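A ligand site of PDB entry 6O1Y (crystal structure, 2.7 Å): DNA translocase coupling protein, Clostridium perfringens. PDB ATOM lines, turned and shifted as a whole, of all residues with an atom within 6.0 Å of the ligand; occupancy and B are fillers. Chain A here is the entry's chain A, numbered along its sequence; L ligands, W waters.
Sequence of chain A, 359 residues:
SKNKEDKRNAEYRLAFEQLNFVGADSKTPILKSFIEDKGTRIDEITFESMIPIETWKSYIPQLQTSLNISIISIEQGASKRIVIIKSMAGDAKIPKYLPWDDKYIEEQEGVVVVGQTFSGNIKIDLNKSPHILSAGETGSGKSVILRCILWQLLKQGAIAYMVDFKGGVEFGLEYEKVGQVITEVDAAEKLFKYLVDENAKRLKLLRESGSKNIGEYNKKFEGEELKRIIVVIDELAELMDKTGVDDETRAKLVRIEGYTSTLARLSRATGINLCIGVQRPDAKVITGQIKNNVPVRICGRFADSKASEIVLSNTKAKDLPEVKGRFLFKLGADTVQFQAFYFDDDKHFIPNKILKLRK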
ATOM      1  N   LYS A  96      -2.422  29.990  27.972  1.00  0.00           N
ATOM      2  CA  LYS A  96      -3.876  30.114  28.004  1.00  0.00           C
ATOM      3  C   LYS A  96      -4.435  30.111  26.566  1.00  0.00           C
ATOM      4  O   LYS A  96      -5.639  29.969  26.335  1.00  0.00           O
ATOM      5  CB  LYS A  96      -4.288  31.406  28.750  1.00  0.00           C
ATOM      6  CG  LYS A  96      -4.195  31.293  30.276  1.00  0.00           C
ATOM      7  CD  LYS A  96      -4.316  32.666  30.981  1.00  0.00           C
ATOM      8  CE  LYS A  96      -2.987  33.407  31.115  1.00  0.00           C
ATOM      9  NZ  LYS A  96      -3.115  34.701  31.831  1.00  0.00           N
ATOM     10  N   TYR A  97      -3.529  30.276  25.596  1.00  0.00           N
ATOM     11  CA  TYR A  97      -3.786  30.290  24.157  1.00  0.00           C
ATOM     12  C   TYR A  97      -2.470  29.946  23.447  1.00  0.00           C
ATOM     13  O   TYR A  97      -1.407  30.493  23.777  1.00  0.00           O
ATOM     14  CB  TYR A  97      -4.354  31.651  23.727  1.00  0.00           C
ATOM     15  CG  TYR A  97      -4.472  31.860  22.226  1.00  0.00           C
ATOM     16  CD1 TYR A  97      -5.479  31.236  21.499  1.00  0.00           C
ATOM     17  CD2 TYR A  97      -3.596  32.710  21.551  1.00  0.00           C
ATOM     18  CE1 TYR A  97      -5.593  31.420  20.125  1.00  0.00           C
ATOM     19  CE2 TYR A  97      -3.708  32.901  20.164  1.00  0.00           C
ATOM     20  CZ  TYR A  97      -4.719  32.264  19.462  1.00  0.00           C
ATOM     21  OH  TYR A  97      -4.873  32.437  18.099  1.00  0.00           O
ATOM     22  N   LEU A  98      -2.548  29.039  22.454  1.00  0.00           N
ATOM     23  CA  LEU A  98      -1.376  28.600  21.697  1.00  0.00           C
ATOM     24  C   LEU A  98      -1.807  28.269  20.260  1.00  0.00           C
ATOM     25  O   LEU A  98      -2.510  27.283  20.081  1.00  0.00           O
ATOM     26  CB  LEU A  98      -0.784  27.376  22.423  1.00  0.00           C
ATOM     27  CG  LEU A  98       0.490  26.723  21.917  1.00  0.00           C
ATOM     28  CD1 LEU A  98       1.635  27.687  21.882  1.00  0.00           C
ATOM     29  CD2 LEU A  98       0.861  25.587  22.785  1.00  0.00           C
ATOM     30  N   GLY A 136     -15.622  16.483  24.214  1.00  0.00           N
ATOM     31  CA  GLY A 136     -15.887  17.799  24.770  1.00  0.00           C
ATOM     32  C   GLY A 136     -17.155  18.444  24.267  1.00  0.00           C
ATOM     33  O   GLY A 136     -17.590  18.161  23.137  1.00  0.00           O
ATOM     34  N   GLU A 137     -17.745  19.339  25.092  1.00  0.00           N
ATOM     35  CA  GLU A 137     -18.970  20.123  24.800  1.00  0.00           C
ATOM     36  C   GLU A 137     -18.854  20.952  23.490  1.00  0.00           C
ATOM     37  O   GLU A 137     -17.748  21.122  22.962  1.00  0.00           O
ATOM     38  CB  GLU A 137     -19.313  21.038  26.003  1.00  0.00           C
ATOM     39  CG  GLU A 137     -19.892  20.309  27.205  1.00  0.00           C
ATOM     40  CD  GLU A 137     -19.467  20.799  28.583  1.00  0.00           C
ATOM     41  OE1 GLU A 137     -18.832  21.874  28.668  1.00  0.00           O
ATOM     42  OE2 GLU A 137     -19.775  20.108  29.575  1.00  0.00           O
ATOM     43  N   THR A 138     -19.988  21.460  22.966  1.00  0.00           N
ATOM     44  CA  THR A 138     -19.965  22.265  21.749  1.00  0.00           C
ATOM     45  C   THR A 138     -19.135  23.522  22.014  1.00  0.00           C
ATOM     46  O   THR A 138     -19.348  24.193  23.026  1.00  0.00           O
ATOM     47  CB  THR A 138     -21.371  22.598  21.257  1.00  0.00           C
ATOM     48  OG1 THR A 138     -22.238  21.500  21.504  1.00  0.00           O
ATOM     49  CG2 THR A 138     -21.407  22.937  19.779  1.00  0.00           C
ATOM     50  N   GLY A 139     -18.154  23.773  21.147  1.00  0.00           N
ATOM     51  CA  GLY A 139     -17.269  24.933  21.243  1.00  0.00           C
ATOM     52  C   GLY A 139     -16.017  24.732  22.062  1.00  0.00           C
ATOM     53  O   GLY A 139     -15.218  25.674  22.192  1.00  0.00           O
ATOM     54  N   SER A 140     -15.803  23.516  22.627  1.00  0.00           N
ATOM     55  CA  SER A 140     -14.612  23.172  23.419  1.00  0.00           C
ATOM     56  C   SER A 140     -13.349  23.143  22.558  1.00  0.00           C
ATOM     57  O   SER A 140     -12.276  23.551  23.009  1.00  0.00           O
ATOM     58  CB  SER A 140     -14.795  21.846  24.162  1.00  0.00           C
ATOM     59  OG  SER A 140     -15.099  20.778  23.283  1.00  0.00           O
ATOM     60  N   GLY A 141     -13.510  22.710  21.309  1.00  0.00           N
ATOM     61  CA  GLY A 141     -12.430  22.636  20.341  1.00  0.00           C
ATOM     62  C   GLY A 141     -11.930  21.241  20.112  1.00  0.00           C
ATOM     63  O   GLY A 141     -10.754  21.053  19.788  1.00  0.00           O
ATOM     64  N   LYS A 142     -12.806  20.250  20.304  1.00  0.00           N
ATOM     65  CA  LYS A 142     -12.487  18.837  20.106  1.00  0.00           C
ATOM     66  C   LYS A 142     -12.311  18.534  18.613  1.00  0.00           C
ATOM     67  O   LYS A 142     -11.521  17.644  18.255  1.00  0.00           O
ATOM     68  CB  LYS A 142     -13.496  17.909  20.804  1.00  0.00           C
ATOM     69  CG  LYS A 142     -14.951  18.085  20.396  1.00  0.00           C
ATOM     70  CD  LYS A 142     -15.762  16.815  20.604  1.00  0.00           C
ATOM     71  CE  LYS A 142     -16.992  16.818  19.750  1.00  0.00           C
ATOM     72  NZ  LYS A 142     -16.675  16.966  18.301  1.00  0.00           N
ATOM     73  N   SER A 143     -13.001  19.302  17.741  1.00  0.00           N
ATOM     74  CA  SER A 143     -12.871  19.197  16.287  1.00  0.00           C
ATOM     75  C   SER A 143     -11.515  19.747  15.872  1.00  0.00           C
ATOM     76  O   SER A 143     -10.803  19.072  15.137  1.00  0.00           O
ATOM     77  CB  SER A 143     -13.975  19.980  15.571  1.00  0.00           C
ATOM     78  OG  SER A 143     -13.825  20.098  14.165  1.00  0.00           O
ATOM     79  N   VAL A 144     -11.159  20.961  16.358  1.00  0.00           N
ATOM     80  CA  VAL A 144      -9.878  21.642  16.095  1.00  0.00           C
ATOM     81  C   VAL A 144      -8.671  20.659  16.245  1.00  0.00           C
ATOM     82  O   VAL A 144      -7.803  20.605  15.373  1.00  0.00           O
ATOM     83  CB  VAL A 144      -9.749  22.943  16.960  1.00  0.00           C
ATOM     84  CG1 VAL A 144      -8.287  23.315  17.229  1.00  0.00           C
ATOM     85  CG2 VAL A 144     -10.474  24.111  16.310  1.00  0.00           C
ATOM     86  N   ILE A 145      -8.668  19.863  17.324  1.00  0.00           N
ATOM     87  CA  ILE A 145      -7.591  18.932  17.597  1.00  0.00           C
ATOM     88  C   ILE A 145      -7.464  17.964  16.465  1.00  0.00           C
ATOM     89  O   ILE A 145      -6.382  17.801  15.916  1.00  0.00           O
ATOM     90  CB  ILE A 145      -7.813  18.187  18.936  1.00  0.00           C
ATOM     91  CG1 ILE A 145      -7.907  19.166  20.121  1.00  0.00           C
ATOM     92  CG2 ILE A 145      -6.713  17.117  19.150  1.00  0.00           C
ATOM     93  CD1 ILE A 145      -7.961  18.517  21.455  1.00  0.00           C
ATOM     94  N   ARG A 147      -8.625  17.990  13.370  1.00  0.00           N
ATOM     95  CA  ARG A 147      -8.234  18.711  12.146  1.00  0.00           C
ATOM     96  C   ARG A 147      -6.711  18.907  12.079  1.00  0.00           C
ATOM     97  O   ARG A 147      -6.133  18.909  10.973  1.00  0.00           O
ATOM     98  CB  ARG A 147      -8.898  20.102  12.104  1.00  0.00           C
ATOM     99  CG  ARG A 147     -10.415  20.082  12.133  1.00  0.00           C
ATOM    100  CD  ARG A 147     -10.985  21.277  11.435  1.00  0.00           C
ATOM    101  NE  ARG A 147     -11.745  22.112  12.360  1.00  0.00           N
ATOM    102  CZ  ARG A 147     -12.871  22.747  12.042  1.00  0.00           C
ATOM    103  NH1 ARG A 147     -13.398  22.634  10.828  1.00  0.00           N
ATOM    104  NH2 ARG A 147     -13.504  23.483  12.958  1.00  0.00           N
ATOM    105  N   GLU A 170     -18.796  20.128   8.245  1.00  0.00           N
ATOM    106  CA  GLU A 170     -17.588  20.229   9.064  1.00  0.00           C
ATOM    107  C   GLU A 170     -16.356  19.809   8.271  1.00  0.00           C
ATOM    108  O   GLU A 170     -15.231  20.031   8.732  1.00  0.00           O
ATOM    109  CB  GLU A 170     -17.723  19.435  10.383  1.00  0.00           C
ATOM    110  CG  GLU A 170     -18.345  20.230  11.524  1.00  0.00           C
ATOM    111  CD  GLU A 170     -17.407  21.255  12.154  1.00  0.00           C
ATOM    112  OE1 GLU A 170     -16.206  20.939  12.347  1.00  0.00           O
ATOM    113  OE2 GLU A 170     -17.881  22.381  12.465  1.00  0.00           O
ATOM    114  N   ASP A 234     -16.225  12.686  13.062  1.00  0.00           N
ATOM    115  CA  ASP A 234     -16.664  13.913  13.750  1.00  0.00           C
ATOM    116  C   ASP A 234     -17.547  13.649  14.964  1.00  0.00           C
ATOM    117  O   ASP A 234     -17.432  14.344  15.984  1.00  0.00           O
ATOM    118  CB  ASP A 234     -17.390  14.858  12.782  1.00  0.00           C
ATOM    119  CG  ASP A 234     -17.691  16.214  13.420  1.00  0.00           C
ATOM    120  OD1 ASP A 234     -16.748  17.053  13.516  1.00  0.00           O
ATOM    121  OD2 ASP A 234     -18.836  16.405  13.859  1.00  0.00           O
ATOM    122  N   LYS A 324     -10.428  28.132  26.954  1.00  0.00           N
ATOM    123  CA  LYS A 324     -10.697  27.639  25.594  1.00  0.00           C
ATOM    124  C   LYS A 324      -9.497  26.943  25.042  1.00  0.00           C
ATOM    125  O   LYS A 324      -8.434  27.564  24.863  1.00  0.00           O
ATOM    126  CB  LYS A 324     -11.108  28.781  24.656  1.00  0.00           C
ATOM    127  CG  LYS A 324     -12.332  28.470  23.813  1.00  0.00           C
ATOM    128  CD  LYS A 324     -13.086  29.761  23.442  1.00  0.00           C
ATOM    129  CE  LYS A 324     -13.726  30.495  24.620  1.00  0.00           C
ATOM    130  NZ  LYS A 324     -13.834  31.962  24.358  1.00  0.00           N
ATOM    131  N   GLY A 325      -9.652  25.640  24.830  1.00  0.00           N
ATOM    132  CA  GLY A 325      -8.606  24.777  24.295  1.00  0.00           C
ATOM    133  C   GLY A 325      -7.829  24.038  25.348  1.00  0.00           C
ATOM    134  O   GLY A 325      -6.852  23.363  25.023  1.00  0.00           O
ATOM    135  N   ARG A 326      -8.248  24.161  26.620  1.00  0.00           N
ATOM    136  CA  ARG A 326      -7.598  23.460  27.730  1.00  0.00           C
ATOM    137  C   ARG A 326      -8.298  22.119  27.910  1.00  0.00           C
ATOM    138  O   ARG A 326      -9.517  22.048  28.194  1.00  0.00           O
ATOM    139  CB  ARG A 326      -7.572  24.297  29.012  1.00  0.00           C
ATOM    140  CG  ARG A 326      -6.699  23.771  30.146  1.00  0.00           C
ATOM    141  CD  ARG A 326      -5.195  23.924  29.910  1.00  0.00           C
ATOM    142  NE  ARG A 326      -4.707  25.281  29.619  1.00  0.00           N
ATOM    143  CZ  ARG A 326      -4.480  26.217  30.532  1.00  0.00           C
ATOM    144  NH1 ARG A 326      -4.818  26.019  31.801  1.00  0.00           N
ATOM    145  NH2 ARG A 326      -4.001  27.392  30.169  1.00  0.00           N
ATOM    146  N   PHE A 327      -7.521  21.054  27.655  1.00  0.00           N
ATOM    147  CA  PHE A 327      -7.945  19.667  27.702  1.00  0.00           C
ATOM    148  C   PHE A 327      -7.184  18.852  28.700  1.00  0.00           C
ATOM    149  O   PHE A 327      -6.176  19.263  29.281  1.00  0.00           O
ATOM    150  CB  PHE A 327      -7.782  19.025  26.302  1.00  0.00           C
ATOM    151  CG  PHE A 327      -8.849  19.416  25.327  1.00  0.00           C
ATOM    152  CD1 PHE A 327      -8.699  20.516  24.507  1.00  0.00           C
ATOM    153  CD2 PHE A 327     -10.040  18.712  25.255  1.00  0.00           C
ATOM    154  CE1 PHE A 327      -9.705  20.909  23.627  1.00  0.00           C
ATOM    155  CE2 PHE A 327     -11.051  19.107  24.392  1.00  0.00           C
ATOM    156  CZ  PHE A 327     -10.886  20.216  23.588  1.00  0.00           C
ATOM    157  N   GLN A 339      -2.734  22.294  26.892  1.00  0.00           N
ATOM    158  CA  GLN A 339      -3.375  23.320  26.094  1.00  0.00           C
ATOM    159  C   GLN A 339      -3.252  22.922  24.627  1.00  0.00           C
ATOM    160  O   GLN A 339      -2.162  22.942  24.052  1.00  0.00           O
ATOM    161  CB  GLN A 339      -2.758  24.731  26.376  1.00  0.00           C
ATOM    162  CG  GLN A 339      -3.267  25.888  25.470  1.00  0.00           C
ATOM    163  CD  GLN A 339      -4.735  26.244  25.598  1.00  0.00           C
ATOM    164  OE1 GLN A 339      -5.393  26.061  26.644  1.00  0.00           O
ATOM    165  NE2 GLN A 339      -5.294  26.790  24.516  1.00  0.00           N
ATOM    166  N   ALA A 340      -4.390  22.558  24.034  1.00  0.00           N
ATOM    167  CA  ALA A 340      -4.463  22.175  22.615  1.00  0.00           C
ATOM    168  C   ALA A 340      -4.138  23.370  21.700  1.00  0.00           C
ATOM    169  O   ALA A 340      -4.616  24.484  21.936  1.00  0.00           O
ATOM    170  CB  ALA A 340      -5.841  21.622  22.299  1.00  0.00           C
ATOM    171  N   PHE A 341      -3.290  23.132  20.678  1.00  0.00           N
ATOM    172  CA  PHE A 341      -2.932  24.141  19.686  1.00  0.00           C
ATOM    173  C   PHE A 341      -4.224  24.589  19.009  1.00  0.00           C
ATOM    174  O   PHE A 341      -5.155  23.784  18.876  1.00  0.00           O
ATOM    175  CB  PHE A 341      -2.031  23.525  18.582  1.00  0.00           C
ATOM    176  CG  PHE A 341      -0.678  22.981  18.952  1.00  0.00           C
ATOM    177  CD1 PHE A 341       0.213  23.737  19.700  1.00  0.00           C
ATOM    178  CD2 PHE A 341      -0.245  21.759  18.464  1.00  0.00           C
ATOM    179  CE1 PHE A 341       1.487  23.248  20.013  1.00  0.00           C
ATOM    180  CE2 PHE A 341       1.034  21.285  18.753  1.00  0.00           C
ATOM    181  CZ  PHE A 341       1.892  22.035  19.533  1.00  0.00           C
ATOM    182  N   TYR A 342      -4.307  25.857  18.614  1.00  0.00           N
ATOM    183  CA  TYR A 342      -5.492  26.317  17.906  1.00  0.00           C
ATOM    184  C   TYR A 342      -5.203  26.200  16.440  1.00  0.00           C
ATOM    185  O   TYR A 342      -4.307  26.864  15.917  1.00  0.00           O
ATOM    186  CB  TYR A 342      -5.965  27.723  18.326  1.00  0.00           C
ATOM    187  CG  TYR A 342      -7.185  28.187  17.556  1.00  0.00           C
ATOM    188  CD1 TYR A 342      -8.279  27.345  17.364  1.00  0.00           C
ATOM    189  CD2 TYR A 342      -7.246  29.466  17.014  1.00  0.00           C
ATOM    190  CE1 TYR A 342      -9.378  27.749  16.598  1.00  0.00           C
ATOM    191  CE2 TYR A 342      -8.345  29.893  16.277  1.00  0.00           C
ATOM    192  CZ  TYR A 342      -9.410  29.027  16.061  1.00  0.00           C
ATOM    193  OH  TYR A 342     -10.493  29.426  15.320  1.00  0.00           O
ATOM    194  N   PHE A 343      -5.916  25.299  15.797  1.00  0.00           N
ATOM    195  CA  PHE A 343      -5.789  25.009  14.377  1.00  0.00           C
ATOM    196  C   PHE A 343      -6.912  25.710  13.644  1.00  0.00           C
ATOM    197  O   PHE A 343      -8.050  25.255  13.641  1.00  0.00           O
ATOM    198  CB  PHE A 343      -5.794  23.490  14.127  1.00  0.00           C
ATOM    199  CG  PHE A 343      -5.531  23.151  12.679  1.00  0.00           C
ATOM    200  CD1 PHE A 343      -6.588  22.953  11.798  1.00  0.00           C
ATOM    201  CD2 PHE A 343      -4.235  23.099  12.182  1.00  0.00           C
ATOM    202  CE1 PHE A 343      -6.346  22.685  10.453  1.00  0.00           C
ATOM    203  CE2 PHE A 343      -4.003  22.819  10.852  1.00  0.00           C
ATOM    204  CZ  PHE A 343      -5.059  22.620   9.996  1.00  0.00           C
HETATM  205  P1  LIG L   1     -17.294  20.276  16.371  1.00  0.00           P
HETATM  206  O1  LIG L   1     -17.049  21.212  15.219  1.00  0.00           O
HETATM  207  O2  LIG L   1     -16.895  18.811  16.035  1.00  0.00           O
HETATM  208  O3  LIG L   1     -18.765  20.273  16.813  1.00  0.00           O
HETATM  209  P2  LIG L   1     -16.476  21.812  18.771  1.00  0.00           P
HETATM  210  O4  LIG L   1     -16.306  21.182  20.107  1.00  0.00           O
HETATM  211  O5  LIG L   1     -17.839  22.502  18.698  1.00  0.00           O
HETATM  212  O6  LIG L   1     -16.410  20.685  17.645  1.00  0.00           O
HETATM  213  P3  LIG L   1     -14.657  23.649  17.345  1.00  0.00           P
HETATM  214  O7  LIG L   1     -15.488  23.512  16.121  1.00  0.00           O
HETATM  215  O8  LIG L   1     -13.335  22.902  17.165  1.00  0.00           O
HETATM  216  O9  LIG L   1     -15.372  22.954  18.584  1.00  0.00           O
HETATM  217  O10 LIG L   1     -14.305  25.217  17.570  1.00  0.00           O
HETATM  218  C1  LIG L   1     -14.675  25.948  18.762  1.00  0.00           C
HETATM  219  C2  LIG L   1     -14.083  27.334  18.786  1.00  0.00           C
HETATM  220  O11 LIG L   1     -13.522  27.598  20.085  1.00  0.00           O
HETATM  221  C3  LIG L   1     -12.952  27.637  17.795  1.00  0.00           C
HETATM  222  O12 LIG L   1     -13.425  27.990  16.502  1.00  0.00           O
HETATM  223  C4  LIG L   1     -12.227  28.777  18.519  1.00  0.00           C
HETATM  224  O13 LIG L   1     -12.868  30.044  18.385  1.00  0.00           O
HETATM  225  C5  LIG L   1     -12.281  28.267  19.956  1.00  0.00           C
HETATM  226  N1  LIG L   1     -11.189  27.346  20.295  1.00  0.00           N
HETATM  227  C6  LIG L   1     -11.091  26.018  19.982  1.00  0.00           C
HETATM  228  N2  LIG L   1      -9.915  25.486  20.278  1.00  0.00           N
HETATM  229  C7  LIG L   1      -9.213  26.548  20.829  1.00  0.00           C
HETATM  230  C8  LIG L   1      -7.886  26.662  21.290  1.00  0.00           C
HETATM  231  N3  LIG L   1      -7.012  25.659  21.278  1.00  0.00           N
HETATM  232  N4  LIG L   1      -7.475  27.875  21.726  1.00  0.00           N
HETATM  233  C9  LIG L   1      -8.340  28.890  21.722  1.00  0.00           C
HETATM  234  N5  LIG L   1      -9.622  28.902  21.308  1.00  0.00           N
HETATM  235  C10 LIG L   1      -9.990  27.691  20.856  1.00  0.00           C
HETATM  236  O   HOH W   1     -12.279  28.133  13.716  1.00  0.00           O
HETATM  237  O   HOH W   2     -11.975  32.264  16.476  1.00  0.00           O
HETATM  238  O   HOH W   3     -19.332  24.895  17.892  1.00  0.00           O
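The backbone carbonyl oxygen (O) of Ala 340 sits at hydrogen-bond distance from a nitrogen (N3) of the ligand (2.7 Å).
N of Gly 139 is in hydrogen-bond range of O5 of the ligand (2.8 Å).
The side-chain amino group of Lys 142 is in salt-bridge range of an oxygen (O2) of the ligand.
O1 of the ligand sits close to OE1 of Glu 170 (3.0 Å).
O8 of the ligand sits at hydrogen-bond distance from N of Val 144 (3.0 Å).
The side-chain carboxylate of Asp 234 sits close to an oxygen (O2) of the ligand (3.1 Å).
An oxygen (O9) of the ligand lies within hydrogen-bond range of the backbone NH of Gly 141 (3.3 Å).
N of Ser 140 is in hydrogen-bond range of O4 of the ligand (3.5 Å).
OG of Ser 140 sits at hydrogen-bond distance from O4 of the ligand (3.4 Å).
O12 of the ligand sits at hydrogen-bond distance from OH of Tyr 342 (3.5 Å).
An oxygen (O7) of the ligand lies within salt-bridge range of the guanidinium group (NH2) of Arg 147, at 3.7 Å.
The backbone carbonyl oxygen (O) of Gly 325 sits at hydrogen-bond distance from the backbone NH (N) of Ala 340 (2.8 Å).
The side-chain hydroxyl of Ser 143 sits at hydrogen-bond distance from the side-chain carboxylate of Glu 170 (3.1 Å).
The side-chain carboxylate (OE1) of Glu 170 lies within salt-bridge range of the guanidinium group (NH1) of Arg 147, at 3.6 Å.
OG of Ser 143 sits at hydrogen-bond distance from NE of Arg 147, 3.4 Å away.
O of Glu 137 is in hydrogen-bond range of OG of Ser 140.
NE2 of Gln 339 sits at hydrogen-bond distance from O of Lys 324.
N of Tyr 342 sits at hydrogen-bond distance from O of Leu 98, at 2.7 Å.
The side-chain amide oxygen (OE1) of Gln 339 is in hydrogen-bond range of the guanidinium group (NE) of Arg 326 (3.2 Å).
The backbone carbonyl oxygen (O) of Glu 137 lies close to an oxygen (O4) of the ligand.
The backbone carbonyl oxygen (O) of Lys 324 lies close to a nitrogen (N4) of the ligand (3.3 Å).
Residues that only touch the ligand: Ser 143, Gly 325, Phe 341, Thr 138, Gln 339 and Tyr 97.
Hydrophobic or aromatic side chains that line the ligand: Tyr 97, Val 144 and Tyr 342.
Of the 25 residues printed, 18 come within 4 Å of the ligand.
The nearest printed residue that does not touch the ligand is Gly 136 (4.5 Å).
Water W1 lies within hydrogen-bond range of the side-chain hydroxyl (OH) of Tyr 342 (2.7 Å) and an oxygen (O12) of the ligand (3.0 Å).
Water W2 bridges an oxygen (O13) of the ligand (3.1 Å) and the side-chain hydroxyl of Tyr 342 (3.4 Å).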
